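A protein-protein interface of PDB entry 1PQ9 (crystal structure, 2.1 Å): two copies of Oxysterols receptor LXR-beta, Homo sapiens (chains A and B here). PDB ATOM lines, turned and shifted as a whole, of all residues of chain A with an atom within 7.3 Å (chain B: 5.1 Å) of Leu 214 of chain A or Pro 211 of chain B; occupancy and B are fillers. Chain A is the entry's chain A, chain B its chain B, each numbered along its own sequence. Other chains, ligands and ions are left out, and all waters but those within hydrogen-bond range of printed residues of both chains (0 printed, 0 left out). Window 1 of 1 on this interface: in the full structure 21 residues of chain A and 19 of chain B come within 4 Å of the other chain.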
ATOM      1  N   LEU A 155      21.508 -11.463 -34.667  1.00  0.00           N
ATOM      2  CA  LEU A 155      20.189 -11.383 -34.042  1.00  0.00           C
ATOM      3  C   LEU A 155      19.086 -11.891 -34.957  1.00  0.00           C
ATOM      4  O   LEU A 155      18.049 -12.326 -34.471  1.00  0.00           O
ATOM      5  CB  LEU A 155      19.849  -9.950 -33.633  1.00  0.00           C
ATOM      6  CG  LEU A 155      20.407  -9.426 -32.325  1.00  0.00           C
ATOM      7  CD1 LEU A 155      19.910  -8.004 -32.143  1.00  0.00           C
ATOM      8  CD2 LEU A 155      19.990 -10.334 -31.169  1.00  0.00           C
ATOM      9  N   LEU A 165      11.361  -1.788 -34.169  1.00  0.00           N
ATOM     10  CA  LEU A 165      12.549  -1.179 -33.590  1.00  0.00           C
ATOM     11  C   LEU A 165      12.704   0.228 -34.137  1.00  0.00           C
ATOM     12  O   LEU A 165      13.125   1.130 -33.437  1.00  0.00           O
ATOM     13  CB  LEU A 165      13.816  -1.956 -33.935  1.00  0.00           C
ATOM     14  CG  LEU A 165      14.767  -2.515 -32.884  1.00  0.00           C
ATOM     15  CD1 LEU A 165      16.165  -2.722 -33.475  1.00  0.00           C
ATOM     16  CD2 LEU A 165      14.828  -1.773 -31.544  1.00  0.00           C
ATOM     17  N   ILE A 168      10.181   2.508 -32.280  1.00  0.00           N
ATOM     18  CA  ILE A 168      10.681   2.742 -30.931  1.00  0.00           C
ATOM     19  C   ILE A 168      11.785   3.804 -30.943  1.00  0.00           C
ATOM     20  O   ILE A 168      11.798   4.748 -30.135  1.00  0.00           O
ATOM     21  CB  ILE A 168      11.165   1.395 -30.349  1.00  0.00           C
ATOM     22  CG1 ILE A 168       9.991   0.452 -30.113  1.00  0.00           C
ATOM     23  CG2 ILE A 168      11.939   1.582 -29.049  1.00  0.00           C
ATOM     24  CD1 ILE A 168      10.407  -0.999 -29.799  1.00  0.00           C
ATOM     25  N   GLN A 188       5.821   5.793 -27.409  1.00  0.00           N
ATOM     26  CA  GLN A 188       6.795   4.712 -27.525  1.00  0.00           C
ATOM     27  C   GLN A 188       6.312   3.419 -26.895  1.00  0.00           C
ATOM     28  O   GLN A 188       6.563   2.337 -27.435  1.00  0.00           O
ATOM     29  CB  GLN A 188       8.140   5.095 -26.869  1.00  0.00           C
ATOM     30  CG  GLN A 188       9.327   4.196 -27.334  1.00  0.00           C
ATOM     31  CD  GLN A 188      10.635   4.441 -26.610  1.00  0.00           C
ATOM     32  OE1 GLN A 188      11.661   4.758 -27.239  1.00  0.00           O
ATOM     33  NE2 GLN A 188      10.640   4.207 -25.331  1.00  0.00           N
ATOM     34  N   VAL A 192       6.981  -0.706 -27.832  1.00  0.00           N
ATOM     35  CA  VAL A 192       7.781  -1.539 -26.957  1.00  0.00           C
ATOM     36  C   VAL A 192       6.981  -2.785 -26.542  1.00  0.00           C
ATOM     37  O   VAL A 192       7.491  -3.905 -26.630  1.00  0.00           O
ATOM     38  CB  VAL A 192       8.273  -0.760 -25.707  1.00  0.00           C
ATOM     39  CG1 VAL A 192       8.979  -1.698 -24.745  1.00  0.00           C
ATOM     40  CG2 VAL A 192       9.190   0.347 -26.094  1.00  0.00           C
ATOM     41  N   LEU A 195       6.619  -5.196 -29.389  1.00  0.00           N
ATOM     42  CA  LEU A 195       7.849  -5.922 -29.684  1.00  0.00           C
ATOM     43  C   LEU A 195       8.054  -6.994 -28.623  1.00  0.00           C
ATOM     44  O   LEU A 195       8.414  -8.116 -28.935  1.00  0.00           O
ATOM     45  CB  LEU A 195       9.056  -5.007 -29.749  1.00  0.00           C
ATOM     46  CG  LEU A 195      10.362  -5.702 -30.112  1.00  0.00           C
ATOM     47  CD1 LEU A 195      10.293  -6.541 -31.374  1.00  0.00           C
ATOM     48  CD2 LEU A 195      11.431  -4.633 -30.253  1.00  0.00           C
ATOM     49  N   LEU A 196       7.808  -6.638 -27.368  1.00  0.00           N
ATOM     50  CA  LEU A 196       7.938  -7.579 -26.258  1.00  0.00           C
ATOM     51  C   LEU A 196       7.053  -8.783 -26.541  1.00  0.00           C
ATOM     52  O   LEU A 196       7.519  -9.902 -26.541  1.00  0.00           O
ATOM     53  CB  LEU A 196       7.547  -6.884 -24.948  1.00  0.00           C
ATOM     54  CG  LEU A 196       7.554  -7.652 -23.634  1.00  0.00           C
ATOM     55  CD1 LEU A 196       8.831  -8.459 -23.496  1.00  0.00           C
ATOM     56  CD2 LEU A 196       7.406  -6.700 -22.444  1.00  0.00           C
ATOM     57  N   LEU A 208      16.578 -13.404 -23.885  1.00  0.00           N
ATOM     58  CA  LEU A 208      17.530 -12.320 -24.086  1.00  0.00           C
ATOM     59  C   LEU A 208      17.447 -11.687 -25.470  1.00  0.00           C
ATOM     60  O   LEU A 208      18.057 -10.659 -25.701  1.00  0.00           O
ATOM     61  CB  LEU A 208      18.965 -12.799 -23.814  1.00  0.00           C
ATOM     62  CG  LEU A 208      19.372 -13.039 -22.355  1.00  0.00           C
ATOM     63  CD1 LEU A 208      20.880 -13.157 -22.263  1.00  0.00           C
ATOM     64  CD2 LEU A 208      18.876 -11.933 -21.447  1.00  0.00           C
ATOM     65  N   ARG A 209      16.684 -12.277 -26.385  1.00  0.00           N
ATOM     66  CA  ARG A 209      16.496 -11.695 -27.709  1.00  0.00           C
ATOM     67  C   ARG A 209      16.042 -10.232 -27.630  1.00  0.00           C
ATOM     68  O   ARG A 209      16.634  -9.343 -28.220  1.00  0.00           O
ATOM     69  CB  ARG A 209      15.470 -12.512 -28.493  1.00  0.00           C
ATOM     70  CG  ARG A 209      14.975 -11.850 -29.768  1.00  0.00           C
ATOM     71  CD  ARG A 209      14.047 -12.730 -30.620  1.00  0.00           C
ATOM     72  NE  ARG A 209      14.069 -12.310 -32.024  1.00  0.00           N
ATOM     73  CZ  ARG A 209      15.085 -12.538 -32.853  1.00  0.00           C
ATOM     74  NH1 ARG A 209      16.150 -13.240 -32.466  1.00  0.00           N
ATOM     75  NH2 ARG A 209      15.024 -12.093 -34.099  1.00  0.00           N
ATOM     76  N   PHE A 210      14.978 -10.001 -26.890  1.00  0.00           N
ATOM     77  CA  PHE A 210      14.397  -8.691 -26.778  1.00  0.00           C
ATOM     78  C   PHE A 210      15.343  -7.650 -26.128  1.00  0.00           C
ATOM     79  O   PHE A 210      15.562  -6.569 -26.730  1.00  0.00           O
ATOM     80  CB  PHE A 210      13.060  -8.831 -26.070  1.00  0.00           C
ATOM     81  CG  PHE A 210      12.384  -7.544 -25.788  1.00  0.00           C
ATOM     82  CD1 PHE A 210      12.094  -6.674 -26.793  1.00  0.00           C
ATOM     83  CD2 PHE A 210      12.060  -7.200 -24.491  1.00  0.00           C
ATOM     84  CE1 PHE A 210      11.460  -5.472 -26.541  1.00  0.00           C
ATOM     85  CE2 PHE A 210      11.425  -6.002 -24.235  1.00  0.00           C
ATOM     86  CZ  PHE A 210      11.125  -5.140 -25.283  1.00  0.00           C
ATOM     87  N   PRO A 211      15.921  -7.968 -24.963  1.00  0.00           N
ATOM     88  CA  PRO A 211      16.945  -7.112 -24.374  1.00  0.00           C
ATOM     89  C   PRO A 211      18.059  -6.820 -25.375  1.00  0.00           C
ATOM     90  O   PRO A 211      18.563  -5.713 -25.378  1.00  0.00           O
ATOM     91  CB  PRO A 211      17.488  -7.958 -23.191  1.00  0.00           C
ATOM     92  CG  PRO A 211      16.352  -8.851 -22.834  1.00  0.00           C
ATOM     93  CD  PRO A 211      15.639  -9.134 -24.096  1.00  0.00           C
ATOM     94  N   ARG A 212      18.453  -7.815 -26.172  1.00  0.00           N
ATOM     95  CA  ARG A 212      19.596  -7.658 -27.069  1.00  0.00           C
ATOM     96  C   ARG A 212      19.250  -6.633 -28.105  1.00  0.00           C
ATOM     97  O   ARG A 212      20.101  -5.832 -28.486  1.00  0.00           O
ATOM     98  CB  ARG A 212      20.016  -8.988 -27.721  1.00  0.00           C
ATOM     99  CG  ARG A 212      20.905  -9.864 -26.882  1.00  0.00           C
ATOM    100  CD  ARG A 212      21.645 -10.913 -27.704  1.00  0.00           C
ATOM    101  NE  ARG A 212      22.186 -11.989 -26.887  1.00  0.00           N
ATOM    102  CZ  ARG A 212      21.521 -13.093 -26.552  1.00  0.00           C
ATOM    103  NH1 ARG A 212      20.262 -13.288 -26.961  1.00  0.00           N
ATOM    104  NH2 ARG A 212      22.111 -14.009 -25.803  1.00  0.00           N
ATOM    105  N   MET A 213      17.981  -6.603 -28.525  1.00  0.00           N
ATOM    106  CA  MET A 213      17.524  -5.604 -29.481  1.00  0.00           C
ATOM    107  C   MET A 213      17.547  -4.205 -28.912  1.00  0.00           C
ATOM    108  O   MET A 213      18.027  -3.251 -29.549  1.00  0.00           O
ATOM    109  CB  MET A 213      16.097  -5.918 -29.977  1.00  0.00           C
ATOM    110  CG  MET A 213      16.012  -7.108 -30.831  1.00  0.00           C
ATOM    111  SD  MET A 213      14.269  -7.481 -31.258  1.00  0.00           S
ATOM    112  CE  MET A 213      13.897  -6.191 -32.015  1.00  0.00           C
ATOM    113  N   LEU A 214      17.050  -4.062 -27.692  1.00  0.00           N
ATOM    114  CA  LEU A 214      17.072  -2.742 -27.071  1.00  0.00           C
ATOM    115  C   LEU A 214      18.490  -2.260 -26.861  1.00  0.00           C
ATOM    116  O   LEU A 214      18.761  -1.077 -27.007  1.00  0.00           O
ATOM    117  CB  LEU A 214      16.283  -2.719 -25.763  1.00  0.00           C
ATOM    118  CG  LEU A 214      14.810  -3.116 -25.856  1.00  0.00           C
ATOM    119  CD1 LEU A 214      14.218  -2.952 -24.460  1.00  0.00           C
ATOM    120  CD2 LEU A 214      14.006  -2.332 -26.881  1.00  0.00           C
ATOM    121  N   MET A 215      19.416  -3.164 -26.585  1.00  0.00           N
ATOM    122  CA  MET A 215      20.812  -2.786 -26.374  1.00  0.00           C
ATOM    123  C   MET A 215      21.466  -2.198 -27.617  1.00  0.00           C
ATOM    124  O   MET A 215      22.435  -1.465 -27.513  1.00  0.00           O
ATOM    125  CB  MET A 215      21.643  -3.991 -25.937  1.00  0.00           C
ATOM    126  CG  MET A 215      21.296  -4.550 -24.564  1.00  0.00           C
ATOM    127  SD  MET A 215      21.914  -3.540 -23.225  1.00  0.00           S
ATOM    128  CE  MET A 215      23.089  -4.575 -22.529  1.00  0.00           C
ATOM    129  N   LYS A 216      20.957  -2.564 -28.795  1.00  0.00           N
ATOM    130  CA  LYS A 216      21.455  -2.035 -30.050  1.00  0.00           C
ATOM    131  C   LYS A 216      21.044  -0.583 -30.218  1.00  0.00           C
ATOM    132  O   LYS A 216      21.739   0.176 -30.872  1.00  0.00           O
ATOM    133  CB  LYS A 216      20.938  -2.872 -31.245  1.00  0.00           C
ATOM    134  CG  LYS A 216      21.499  -4.286 -31.279  1.00  0.00           C
ATOM    135  CD  LYS A 216      22.943  -4.315 -31.675  1.00  0.00           C
ATOM    136  CE  LYS A 216      23.535  -5.709 -31.481  1.00  0.00           C
ATOM    137  NZ  LYS A 216      24.935  -5.682 -31.044  1.00  0.00           N
ATOM    138  N   LEU A 217      19.910  -0.193 -29.649  1.00  0.00           N
ATOM    139  CA  LEU A 217      19.603   1.240 -29.538  1.00  0.00           C
ATOM    140  C   LEU A 217      20.656   2.013 -28.806  1.00  0.00           C
ATOM    141  O   LEU A 217      20.947   3.132 -29.182  1.00  0.00           O
ATOM    142  CB  LEU A 217      18.229   1.504 -28.921  1.00  0.00           C
ATOM    143  CG  LEU A 217      17.011   0.815 -29.547  1.00  0.00           C
ATOM    144  CD1 LEU A 217      15.789   1.189 -28.742  1.00  0.00           C
ATOM    145  CD2 LEU A 217      16.793   1.181 -30.995  1.00  0.00           C
ATOM    146  N   VAL A 218      21.272   1.424 -27.791  1.00  0.00           N
ATOM    147  CA  VAL A 218      22.383   2.079 -27.079  1.00  0.00           C
ATOM    148  C   VAL A 218      23.520   2.353 -28.054  1.00  0.00           C
ATOM    149  O   VAL A 218      24.050   3.483 -28.134  1.00  0.00           O
ATOM    150  CB  VAL A 218      22.937   1.205 -25.963  1.00  0.00           C
ATOM    151  CG1 VAL A 218      24.037   1.919 -25.186  1.00  0.00           C
ATOM    152  CG2 VAL A 218      21.824   0.785 -25.023  1.00  0.00           C
ATOM    153  N   SER A 219      23.906   1.300 -28.787  1.00  0.00           N
ATOM    154  CA  SER A 219      25.034   1.366 -29.707  1.00  0.00           C
ATOM    155  C   SER A 219      24.747   2.433 -30.743  1.00  0.00           C
ATOM    156  O   SER A 219      25.621   3.174 -31.119  1.00  0.00           O
ATOM    157  CB  SER A 219      25.232   0.023 -30.432  1.00  0.00           C
ATOM    158  OG  SER A 219      25.401  -1.025 -29.520  1.00  0.00           O
ATOM    159  N   LEU A 220      23.501   2.525 -31.171  1.00  0.00           N
ATOM    160  CA  LEU A 220      23.139   3.502 -32.213  1.00  0.00           C
ATOM    161  C   LEU A 220      23.391   4.943 -31.796  1.00  0.00           C
ATOM    162  O   LEU A 220      23.730   5.761 -32.631  1.00  0.00           O
ATOM    163  CB  LEU A 220      21.708   3.324 -32.621  1.00  0.00           C
ATOM    164  CG  LEU A 220      21.464   2.179 -33.600  1.00  0.00           C
ATOM    165  CD1 LEU A 220      19.978   1.941 -33.723  1.00  0.00           C
ATOM    166  CD2 LEU A 220      22.090   2.437 -34.956  1.00  0.00           C
ATOM    167  N   GLN B 207       5.724  -5.703 -16.580  1.00  0.00           N
ATOM    168  CA  GLN B 207       6.568  -6.275 -17.637  1.00  0.00           C
ATOM    169  C   GLN B 207       7.478  -5.246 -18.328  1.00  0.00           C
ATOM    170  O   GLN B 207       8.461  -5.631 -18.954  1.00  0.00           O
ATOM    171  CB  GLN B 207       5.719  -7.004 -18.698  1.00  0.00           C
ATOM    172  CG  GLN B 207       5.459  -8.503 -18.424  1.00  0.00           C
ATOM    173  CD  GLN B 207       6.732  -9.260 -18.048  1.00  0.00           C
ATOM    174  OE1 GLN B 207       6.797  -9.882 -16.980  1.00  0.00           O
ATOM    175  NE2 GLN B 207       7.757  -9.187 -18.911  1.00  0.00           N
ATOM    176  N   LEU B 208       7.165  -3.958 -18.198  1.00  0.00           N
ATOM    177  CA  LEU B 208       7.914  -2.913 -18.896  1.00  0.00           C
ATOM    178  C   LEU B 208       9.060  -2.305 -18.090  1.00  0.00           C
ATOM    179  O   LEU B 208       9.826  -1.522 -18.626  1.00  0.00           O
ATOM    180  CB  LEU B 208       6.969  -1.791 -19.316  1.00  0.00           C
ATOM    181  CG  LEU B 208       6.026  -2.126 -20.461  1.00  0.00           C
ATOM    182  CD1 LEU B 208       5.170  -0.916 -20.712  1.00  0.00           C
ATOM    183  CD2 LEU B 208       6.827  -2.513 -21.695  1.00  0.00           C
ATOM    184  N   ARG B 209       9.193  -2.684 -16.817  1.00  0.00           N
ATOM    185  CA  ARG B 209      10.203  -2.071 -15.944  1.00  0.00           C
ATOM    186  C   ARG B 209      11.590  -2.379 -16.462  1.00  0.00           C
ATOM    187  O   ARG B 209      12.407  -1.484 -16.605  1.00  0.00           O
ATOM    188  CB  ARG B 209      10.038  -2.574 -14.502  1.00  0.00           C
ATOM    189  CG  ARG B 209      11.280  -2.519 -13.627  1.00  0.00           C
ATOM    190  CD  ARG B 209      11.072  -3.195 -12.238  1.00  0.00           C
ATOM    191  NE  ARG B 209      11.875  -2.537 -11.202  1.00  0.00           N
ATOM    192  CZ  ARG B 209      11.630  -1.315 -10.796  1.00  0.00           C
ATOM    193  NH1 ARG B 209      10.605  -0.653 -11.290  1.00  0.00           N
ATOM    194  NH2 ARG B 209      12.401  -0.754  -9.888  1.00  0.00           N
ATOM    195  N   PHE B 210      11.840  -3.641 -16.765  1.00  0.00           N
ATOM    196  CA  PHE B 210      13.127  -4.049 -17.250  1.00  0.00           C
ATOM    197  C   PHE B 210      13.528  -3.336 -18.576  1.00  0.00           C
ATOM    198  O   PHE B 210      14.607  -2.776 -18.648  1.00  0.00           O
ATOM    199  CB  PHE B 210      13.211  -5.572 -17.392  1.00  0.00           C
ATOM    200  CG  PHE B 210      14.552  -6.047 -17.833  1.00  0.00           C
ATOM    201  CD1 PHE B 210      15.657  -5.821 -17.058  1.00  0.00           C
ATOM    202  CD2 PHE B 210      14.714  -6.693 -19.039  1.00  0.00           C
ATOM    203  CE1 PHE B 210      16.896  -6.248 -17.465  1.00  0.00           C
ATOM    204  CE2 PHE B 210      15.951  -7.140 -19.443  1.00  0.00           C
ATOM    205  CZ  PHE B 210      17.034  -6.921 -18.660  1.00  0.00           C
ATOM    206  N   PRO B 211      12.675  -3.356 -19.611  1.00  0.00           N
ATOM    207  CA  PRO B 211      12.948  -2.542 -20.804  1.00  0.00           C
ATOM    208  C   PRO B 211      13.187  -1.084 -20.492  1.00  0.00           C
ATOM    209  O   PRO B 211      14.097  -0.512 -21.071  1.00  0.00           O
ATOM    210  CB  PRO B 211      11.685  -2.716 -21.659  1.00  0.00           C
ATOM    211  CG  PRO B 211      11.168  -4.024 -21.277  1.00  0.00           C
ATOM    212  CD  PRO B 211      11.494  -4.209 -19.807  1.00  0.00           C
ATOM    213  N   ARG B 212      12.396  -0.462 -19.634  1.00  0.00           N
ATOM    214  CA  ARG B 212      12.646   0.948 -19.322  1.00  0.00           C
ATOM    215  C   ARG B 212      14.029   1.145 -18.697  1.00  0.00           C
ATOM    216  O   ARG B 212      14.716   2.132 -18.990  1.00  0.00           O
ATOM    217  CB  ARG B 212      11.580   1.517 -18.413  1.00  0.00           C
ATOM    218  CG  ARG B 212      10.271   1.848 -19.098  1.00  0.00           C
ATOM    219  CD  ARG B 212       9.213   2.294 -18.093  1.00  0.00           C
ATOM    220  NE  ARG B 212       7.852   2.303 -18.608  1.00  0.00           N
ATOM    221  CZ  ARG B 212       6.824   1.619 -18.081  1.00  0.00           C
ATOM    222  NH1 ARG B 212       6.973   0.817 -17.015  1.00  0.00           N
ATOM    223  NH2 ARG B 212       5.629   1.725 -18.642  1.00  0.00           N
ATOM    224  N   MET B 213      14.483   0.175 -17.907  1.00  0.00           N
ATOM    225  CA  MET B 213      15.812   0.266 -17.306  1.00  0.00           C
ATOM    226  C   MET B 213      16.898   0.238 -18.338  1.00  0.00           C
ATOM    227  O   MET B 213      17.842   1.033 -18.294  1.00  0.00           O
ATOM    228  CB  MET B 213      16.046  -0.903 -16.358  1.00  0.00           C
ATOM    229  CG  MET B 213      15.158  -0.844 -15.198  1.00  0.00           C
ATOM    230  SD  MET B 213      15.719  -1.952 -13.865  1.00  0.00           S
ATOM    231  CE  MET B 213      17.180  -1.292 -13.660  1.00  0.00           C
ATOM    232  N   LEU B 214      16.774  -0.704 -19.269  1.00  0.00           N
ATOM    233  CA  LEU B 214      17.718  -0.797 -20.392  1.00  0.00           C
ATOM    234  C   LEU B 214      17.727   0.479 -21.224  1.00  0.00           C
ATOM    235  O   LEU B 214      18.768   0.913 -21.689  1.00  0.00           O
ATOM    236  CB  LEU B 214      17.386  -2.006 -21.286  1.00  0.00           C
ATOM    237  CG  LEU B 214      17.556  -3.385 -20.646  1.00  0.00           C
ATOM    238  CD1 LEU B 214      17.618  -4.439 -21.755  1.00  0.00           C
ATOM    239  CD2 LEU B 214      18.767  -3.494 -19.754  1.00  0.00           C
ATOM    240  N   MET B 215      16.579   1.113 -21.370  1.00  0.00           N
ATOM    241  CA  MET B 215      16.506   2.338 -22.156  1.00  0.00           C
ATOM    242  C   MET B 215      17.193   3.505 -21.442  1.00  0.00           C
ATOM    243  O   MET B 215      17.545   4.496 -22.066  1.00  0.00           O
ATOM    244  CB  MET B 215      15.073   2.701 -22.428  1.00  0.00           C
ATOM    245  CG  MET B 215      14.358   1.672 -23.229  1.00  0.00           C
ATOM    246  SD  MET B 215      14.520   1.867 -24.981  1.00  0.00           S
ATOM    247  CE  MET B 215      12.944   1.478 -25.412  1.00  0.00           C
ATOM    248  N   VAL B 218      20.530   3.884 -22.961  1.00  0.00           N
ATOM    249  CA  VAL B 218      20.473   4.630 -24.193  1.00  0.00           C
ATOM    250  C   VAL B 218      20.611   6.108 -23.865  1.00  0.00           C
ATOM    251  O   VAL B 218      21.429   6.805 -24.459  1.00  0.00           O
ATOM    252  CB  VAL B 218      19.130   4.323 -24.973  1.00  0.00           C
ATOM    253  CG1 VAL B 218      19.013   5.193 -26.219  1.00  0.00           C
ATOM    254  CG2 VAL B 218      19.041   2.831 -25.363  1.00  0.00           C
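The backbone carbonyl oxygen (O) of Ile 168 of chain A sits close to the side-chain amide oxygen (OE1) of Gln 188 of chain A, 2.9 Å away.
Among the printed residues, merely in contact across the chains: Val 218 of chain A with Val 218 of chain B (3.5 Å), Phe 210 of chain A with Pro 211 of chain B (3.6 Å), Gln 188 of chain A with Met 215 of chain B (3.6 Å), Ile 168 of chain A with Met 215 of chain B (3.8 Å), Leu 214 of chain A with Pro 211 of chain B (3.8 Å), Leu 196 of chain A with Gln 207 of chain B (3.8 Å), Pro 211 of chain A with Leu 214 of chain B (3.8 Å), Pro 211 of chain A with Phe 210 of chain B (3.8 Å), Val 192 of chain A with Leu 208 of chain B (3.8 Å), Leu 217 of chain A with Val 218 of chain B (3.9 Å) and Val 192 of chain A with Met 215 of chain B (3.98 Å).
Printed residues of chain B within 4 Å of Phe 210 of chain A: Pro 211. Leu 214 of chain A touches one residue of chain B. Printed residues of chain B within 4 Å of Val 218 of chain A: Val 218. Of the printed residues of chain A, Phe 210 of chain B touches Pro 211 (3.8 Å). Pro 211 of chain B touches just these residues of chain A: Phe 210 (3.6 Å) and Leu 214 (3.8 Å). The nearest printed residue of chain B that does not touch Leu 214 of chain A is Met 215 of chain B (4.2 Å). The nearest residue of chain A that does not touch Pro 211 of chain B is Val 192 of chain A (4.2 Å). The nearest printed residue of chain A that does not touch Val 218 of chain B is Leu 214 of chain A (4.2 Å).
Hydrophobic or aromatic side chains of chain A that line the printed part of chain B: Ile 168, Val 192, Leu 196, Phe 210, Pro 211, Leu 214, Leu 217 and Val 218. Along chain A the printed residues that touch a printed residue of chain B span positions 168 to 218. Of the 10 printed residues of chain B, 7 touch a printed residue of chain A. Hydrophobic or aromatic side chains of chain B within 4 Å of the printed part of chain A: Leu 208, Phe 210, Pro 211, Leu 214, Met 215 and Val 218. Along chain B the printed residues that touch a printed residue of chain A span positions 207 to 218. Among the printed residues, 11 pairs touch across the chains.
Phe 210 of chain A touches Pro 211 of chain B, and with the chains exchanged Pro 211 of chain A touches Phe 210 of chain B. Pro 211 of chain A touches Leu 214 of chain B, and with the chains exchanged Leu 214 of chain A touches Pro 211 of chain B. Val 218 of chain A touches its own counterpart, Val 218 of chain B. Positions printed for both chains: 208, 209, 210, 211, 212, 213, 214, 215 and 218. Of the 11 pairs that touch across the chains among the printed residues, 5 have their exchanged pair printed and touching as well.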
